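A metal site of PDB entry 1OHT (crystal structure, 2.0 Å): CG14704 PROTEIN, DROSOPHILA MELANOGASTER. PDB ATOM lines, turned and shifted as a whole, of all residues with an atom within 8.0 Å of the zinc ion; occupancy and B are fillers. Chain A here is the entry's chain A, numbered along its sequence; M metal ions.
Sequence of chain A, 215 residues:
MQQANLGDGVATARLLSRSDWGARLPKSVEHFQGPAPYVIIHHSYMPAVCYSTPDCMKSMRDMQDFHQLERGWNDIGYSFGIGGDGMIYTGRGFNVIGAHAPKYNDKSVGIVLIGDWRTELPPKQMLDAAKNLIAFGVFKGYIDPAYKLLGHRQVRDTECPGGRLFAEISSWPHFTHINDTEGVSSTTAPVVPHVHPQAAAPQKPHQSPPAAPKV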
ATOM      1  N   ILE A  40       5.136  -8.832   2.117  1.00  0.00           N
ATOM      2  CA  ILE A  40       5.176  -9.858   1.077  1.00  0.00           C
ATOM      3  C   ILE A  40       5.495  -9.170  -0.240  1.00  0.00           C
ATOM      4  O   ILE A  40       4.757  -8.266  -0.685  1.00  0.00           O
ATOM      5  CB  ILE A  40       3.811 -10.586   0.821  1.00  0.00           C
ATOM      6  CG1 ILE A  40       3.114 -11.040   2.118  1.00  0.00           C
ATOM      7  CG2 ILE A  40       4.041 -11.760  -0.123  1.00  0.00           C
ATOM      8  CD1 ILE A  40       3.807 -11.998   2.939  1.00  0.00           C
ATOM      9  N   ILE A  41       6.550  -9.659  -0.885  1.00  0.00           N
ATOM     10  CA  ILE A  41       6.992  -9.108  -2.155  1.00  0.00           C
ATOM     11  C   ILE A  41       6.465  -9.874  -3.330  1.00  0.00           C
ATOM     12  O   ILE A  41       6.478 -11.126  -3.330  1.00  0.00           O
ATOM     13  CB  ILE A  41       8.530  -9.114  -2.232  1.00  0.00           C
ATOM     14  CG1 ILE A  41       9.117  -8.401  -1.002  1.00  0.00           C
ATOM     15  CG2 ILE A  41       8.977  -8.469  -3.531  1.00  0.00           C
ATOM     16  CD1 ILE A  41       8.562  -6.961  -0.823  1.00  0.00           C
ATOM     17  N   HIS A  42       5.996  -9.131  -4.343  1.00  0.00           N
ATOM     18  CA  HIS A  42       5.476  -9.739  -5.556  1.00  0.00           C
ATOM     19  C   HIS A  42       6.088  -8.989  -6.738  1.00  0.00           C
ATOM     20  O   HIS A  42       6.676  -7.905  -6.575  1.00  0.00           O
ATOM     21  CB  HIS A  42       3.960  -9.505  -5.704  1.00  0.00           C
ATOM     22  CG  HIS A  42       3.147  -9.900  -4.505  1.00  0.00           C
ATOM     23  ND1 HIS A  42       2.641 -11.175  -4.350  1.00  0.00           N
ATOM     24  CD2 HIS A  42       2.691  -9.183  -3.456  1.00  0.00           C
ATOM     25  CE1 HIS A  42       1.895 -11.221  -3.262  1.00  0.00           C
ATOM     26  NE2 HIS A  42       1.920 -10.022  -2.694  1.00  0.00           N
ATOM     27  N   HIS A  43       5.945  -9.593  -7.928  1.00  0.00           N
ATOM     28  CA  HIS A  43       6.254  -8.900  -9.181  1.00  0.00           C
ATOM     29  C   HIS A  43       4.904  -9.010  -9.910  1.00  0.00           C
ATOM     30  O   HIS A  43       4.024  -9.804  -9.504  1.00  0.00           O
ATOM     31  CB  HIS A  43       7.445  -9.478  -9.959  1.00  0.00           C
ATOM     32  CG  HIS A  43       7.168 -10.753 -10.710  1.00  0.00           C
ATOM     33  ND1 HIS A  43       8.020 -11.231 -11.673  1.00  0.00           N
ATOM     34  CD2 HIS A  43       6.213 -11.706 -10.562  1.00  0.00           C
ATOM     35  CE1 HIS A  43       7.630 -12.416 -12.081  1.00  0.00           C
ATOM     36  NE2 HIS A  43       6.519 -12.731 -11.423  1.00  0.00           N
ATOM     37  N   SER A  44       4.683  -8.199 -10.945  1.00  0.00           N
ATOM     38  CA  SER A  44       3.394  -8.245 -11.631  1.00  0.00           C
ATOM     39  C   SER A  44       3.378  -9.203 -12.787  1.00  0.00           C
ATOM     40  O   SER A  44       2.294  -9.682 -13.175  1.00  0.00           O
ATOM     41  CB  SER A  44       3.020  -6.865 -12.187  1.00  0.00           C
ATOM     42  OG  SER A  44       3.979  -6.382 -13.106  1.00  0.00           O
ATOM     43  N   TYR A  78      -2.839  -5.463  -4.290  1.00  0.00           N
ATOM     44  CA  TYR A  78      -1.660  -5.159  -3.471  1.00  0.00           C
ATOM     45  C   TYR A  78      -1.813  -3.890  -2.615  1.00  0.00           C
ATOM     46  O   TYR A  78      -2.658  -3.044  -2.882  1.00  0.00           O
ATOM     47  CB  TYR A  78      -0.433  -4.988  -4.368  1.00  0.00           C
ATOM     48  CG  TYR A  78      -0.382  -5.971  -5.526  1.00  0.00           C
ATOM     49  CD1 TYR A  78      -0.847  -5.604  -6.788  1.00  0.00           C
ATOM     50  CD2 TYR A  78       0.169  -7.254  -5.356  1.00  0.00           C
ATOM     51  CE1 TYR A  78      -0.746  -6.476  -7.845  1.00  0.00           C
ATOM     52  CE2 TYR A  78       0.258  -8.134  -6.412  1.00  0.00           C
ATOM     53  CZ  TYR A  78      -0.197  -7.729  -7.660  1.00  0.00           C
ATOM     54  OH  TYR A  78      -0.073  -8.561  -8.754  1.00  0.00           O
ATOM     55  N   HIS A 100      -3.604 -10.477  -2.272  1.00  0.00           N
ATOM     56  CA  HIS A 100      -2.355 -10.788  -2.977  1.00  0.00           C
ATOM     57  C   HIS A 100      -1.666 -11.995  -2.305  1.00  0.00           C
ATOM     58  O   HIS A 100      -0.735 -12.601  -2.859  1.00  0.00           O
ATOM     59  CB  HIS A 100      -1.435  -9.556  -2.876  1.00  0.00           C
ATOM     60  CG  HIS A 100      -1.046  -9.219  -1.472  1.00  0.00           C
ATOM     61  ND1 HIS A 100      -0.007  -9.834  -0.819  1.00  0.00           N
ATOM     62  CD2 HIS A 100      -1.602  -8.380  -0.565  1.00  0.00           C
ATOM     63  CE1 HIS A 100       0.059  -9.395   0.429  1.00  0.00           C
ATOM     64  NE2 HIS A 100      -0.893  -8.502   0.600  1.00  0.00           N
ATOM     65  N   ALA A 101      -2.058 -12.325  -1.080  1.00  0.00           N
ATOM     66  CA  ALA A 101      -1.449 -13.462  -0.417  1.00  0.00           C
ATOM     67  C   ALA A 101      -2.373 -14.140   0.592  1.00  0.00           C
ATOM     68  O   ALA A 101      -2.494 -13.705   1.720  1.00  0.00           O
ATOM     69  CB  ALA A 101      -0.112 -13.073   0.242  1.00  0.00           C
ATOM     70  N   ILE A 111       3.663  -5.727  -1.520  1.00  0.00           N
ATOM     71  CA  ILE A 111       4.328  -4.767  -2.393  1.00  0.00           C
ATOM     72  C   ILE A 111       4.637  -5.416  -3.740  1.00  0.00           C
ATOM     73  O   ILE A 111       5.309  -6.471  -3.827  1.00  0.00           O
ATOM     74  CB  ILE A 111       5.665  -4.313  -1.756  1.00  0.00           C
ATOM     75  CG1 ILE A 111       5.392  -3.795  -0.331  1.00  0.00           C
ATOM     76  CG2 ILE A 111       6.322  -3.210  -2.607  1.00  0.00           C
ATOM     77  CD1 ILE A 111       6.640  -3.355   0.418  1.00  0.00           C
ATOM     78  N   VAL A 112       4.146  -4.817  -4.822  1.00  0.00           N
ATOM     79  CA  VAL A 112       4.411  -5.420  -6.115  1.00  0.00           C
ATOM     80  C   VAL A 112       5.357  -4.555  -6.916  1.00  0.00           C
ATOM     81  O   VAL A 112       5.121  -3.359  -7.140  1.00  0.00           O
ATOM     82  CB  VAL A 112       3.089  -5.659  -6.947  1.00  0.00           C
ATOM     83  CG1 VAL A 112       2.416  -4.347  -7.210  1.00  0.00           C
ATOM     84  CG2 VAL A 112       3.426  -6.377  -8.287  1.00  0.00           C
ATOM     85  N   GLY A 151       8.674 -13.657   0.053  1.00  0.00           N
ATOM     86  CA  GLY A 151       8.295 -13.522  -1.335  1.00  0.00           C
ATOM     87  C   GLY A 151       7.005 -14.332  -1.399  1.00  0.00           C
ATOM     88  O   GLY A 151       6.821 -15.260  -0.603  1.00  0.00           O
ATOM     89  N   HIS A 152       6.122 -13.990  -2.325  1.00  0.00           N
ATOM     90  CA  HIS A 152       4.851 -14.677  -2.506  1.00  0.00           C
ATOM     91  C   HIS A 152       5.018 -16.230  -2.631  1.00  0.00           C
ATOM     92  O   HIS A 152       4.184 -16.985  -2.114  1.00  0.00           O
ATOM     93  CB  HIS A 152       4.189 -14.109  -3.774  1.00  0.00           C
ATOM     94  CG  HIS A 152       2.783 -14.563  -4.005  1.00  0.00           C
ATOM     95  ND1 HIS A 152       2.041 -14.161  -5.104  1.00  0.00           N
ATOM     96  CD2 HIS A 152       1.966 -15.385  -3.296  1.00  0.00           C
ATOM     97  CE1 HIS A 152       0.853 -14.717  -5.063  1.00  0.00           C
ATOM     98  NE2 HIS A 152       0.774 -15.465  -3.979  1.00  0.00           N
ATOM     99  N   ARG A 153       6.076 -16.699  -3.284  1.00  0.00           N
ATOM    100  CA  ARG A 153       6.264 -18.157  -3.469  1.00  0.00           C
ATOM    101  C   ARG A 153       6.386 -18.944  -2.173  1.00  0.00           C
ATOM    102  O   ARG A 153       6.115 -20.145  -2.140  1.00  0.00           O
ATOM    103  CB  ARG A 153       7.487 -18.434  -4.319  1.00  0.00           C
ATOM    104  CG  ARG A 153       8.786 -17.884  -3.724  1.00  0.00           C
ATOM    105  CD  ARG A 153       9.989 -18.427  -4.467  1.00  0.00           C
ATOM    106  NE  ARG A 153       9.937 -18.056  -5.874  1.00  0.00           N
ATOM    107  CZ  ARG A 153      10.881 -18.335  -6.780  1.00  0.00           C
ATOM    108  NH1 ARG A 153      11.990 -19.012  -6.450  1.00  0.00           N
ATOM    109  NH2 ARG A 153      10.727 -17.877  -8.028  1.00  0.00           N
ATOM    110  N   VAL A 155       4.524 -18.567   0.434  1.00  0.00           N
ATOM    111  CA  VAL A 155       3.253 -18.799   1.145  1.00  0.00           C
ATOM    112  C   VAL A 155       2.146 -19.414   0.281  1.00  0.00           C
ATOM    113  O   VAL A 155       1.078 -19.792   0.772  1.00  0.00           O
ATOM    114  CB  VAL A 155       2.738 -17.490   1.748  1.00  0.00           C
ATOM    115  CG1 VAL A 155       3.844 -16.873   2.602  1.00  0.00           C
ATOM    116  CG2 VAL A 155       2.277 -16.543   0.641  1.00  0.00           C
ATOM    117  N   ARG A 156       2.431 -19.497  -1.000  1.00  0.00           N
ATOM    118  CA  ARG A 156       1.517 -20.040  -1.980  1.00  0.00           C
ATOM    119  C   ARG A 156       2.332 -20.703  -3.057  1.00  0.00           C
ATOM    120  O   ARG A 156       3.540 -20.472  -3.190  1.00  0.00           O
ATOM    121  CB  ARG A 156       0.692 -18.919  -2.617  1.00  0.00           C
ATOM    122  CG  ARG A 156      -0.554 -18.584  -1.858  1.00  0.00           C
ATOM    123  CD  ARG A 156      -1.646 -19.529  -2.313  1.00  0.00           C
ATOM    124  NE  ARG A 156      -1.952 -20.542  -1.330  1.00  0.00           N
ATOM    125  CZ  ARG A 156      -2.411 -21.744  -1.629  1.00  0.00           C
ATOM    126  NH1 ARG A 156      -2.600 -22.112  -2.901  1.00  0.00           N
ATOM    127  NH2 ARG A 156      -2.694 -22.587  -0.656  1.00  0.00           N
ATOM    128  N   THR A 158       3.335 -20.613  -6.291  1.00  0.00           N
ATOM    129  CA  THR A 158       3.462 -19.708  -7.408  1.00  0.00           C
ATOM    130  C   THR A 158       4.949 -19.442  -7.592  1.00  0.00           C
ATOM    131  O   THR A 158       5.757 -19.710  -6.706  1.00  0.00           O
ATOM    132  CB  THR A 158       2.760 -18.360  -7.122  1.00  0.00           C
ATOM    133  OG1 THR A 158       3.190 -17.367  -8.082  1.00  0.00           O
ATOM    134  CG2 THR A 158       3.103 -17.859  -5.708  1.00  0.00           C
ATOM    135  N   GLU A 159       5.286 -18.891  -8.737  1.00  0.00           N
ATOM    136  CA  GLU A 159       6.643 -18.561  -9.037  1.00  0.00           C
ATOM    137  C   GLU A 159       6.959 -17.139  -8.565  1.00  0.00           C
ATOM    138  O   GLU A 159       8.127 -16.752  -8.446  1.00  0.00           O
ATOM    139  CB  GLU A 159       6.812 -18.685 -10.534  1.00  0.00           C
ATOM    140  CG  GLU A 159       8.177 -18.457 -11.043  1.00  0.00           C
ATOM    141  CD  GLU A 159       8.258 -18.694 -12.545  1.00  0.00           C
ATOM    142  OE1 GLU A 159       9.347 -18.457 -13.109  1.00  0.00           O
ATOM    143  OE2 GLU A 159       7.233 -19.109 -13.166  1.00  0.00           O
ATOM    144  N   CYS A 160       5.916 -16.361  -8.297  1.00  0.00           N
ATOM    145  CA  CYS A 160       6.053 -14.977  -7.859  1.00  0.00           C
ATOM    146  C   CYS A 160       6.942 -14.933  -6.623  1.00  0.00           C
ATOM    147  O   CYS A 160       6.792 -15.776  -5.728  1.00  0.00           O
ATOM    148  CB  CYS A 160       4.684 -14.409  -7.529  1.00  0.00           C
ATOM    149  SG  CYS A 160       4.744 -12.667  -7.079  1.00  0.00           S
ATOM    150  N   PRO A 161       7.801 -13.906  -6.502  1.00  0.00           N
ATOM    151  CA  PRO A 161       8.083 -12.727  -7.345  1.00  0.00           C
ATOM    152  C   PRO A 161       9.155 -12.874  -8.401  1.00  0.00           C
ATOM    153  O   PRO A 161       9.801 -11.880  -8.727  1.00  0.00           O
ATOM    154  CB  PRO A 161       8.511 -11.673  -6.330  1.00  0.00           C
ATOM    155  CG  PRO A 161       9.385 -12.552  -5.389  1.00  0.00           C
ATOM    156  CD  PRO A 161       8.578 -13.829  -5.237  1.00  0.00           C
ATOM    157  N   GLY A 162       9.342 -14.074  -8.936  1.00  0.00           N
ATOM    158  CA  GLY A 162      10.361 -14.277  -9.932  1.00  0.00           C
ATOM    159  C   GLY A 162      11.637 -14.774  -9.252  1.00  0.00           C
ATOM    160  O   GLY A 162      11.966 -14.336  -8.161  1.00  0.00           O
HETATM  161 ZN    ZN M   1       2.646 -12.460  -6.106  1.00  0.00          ZN
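NE2 of His 42 is in hydrogen-bond range of ND1 of His 100 (2.7 Å).
The backbone carbonyl oxygen (O) of Cys 160 is in hydrogen-bond range of the backbone NH (N) of Arg 153, 2.7 Å away.
A ring nitrogen (NE2) of His 152 is in hydrogen-bond range of the backbone carbonyl oxygen of His 100.
O of Ile 41 sits at hydrogen-bond distance from N of His 152.
The backbone NH of Cys 160 is in hydrogen-bond range of the side-chain hydroxyl of Thr 158 (2.9 Å).
The backbone NH (N) of His 43 lies close to the side-chain sulfur (SG) of Cys 160.
The backbone NH of His 42 is in hydrogen-bond range of the backbone carbonyl oxygen of Ile 111 (2.8 Å).
The zinc ion is bound by ND1 of His 152 (2.1 Å).
ND1 of His 42 binds the zinc ion, 2.2 Å away.
SG of Cys 160 is bound to the zinc ion (2.3 Å).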
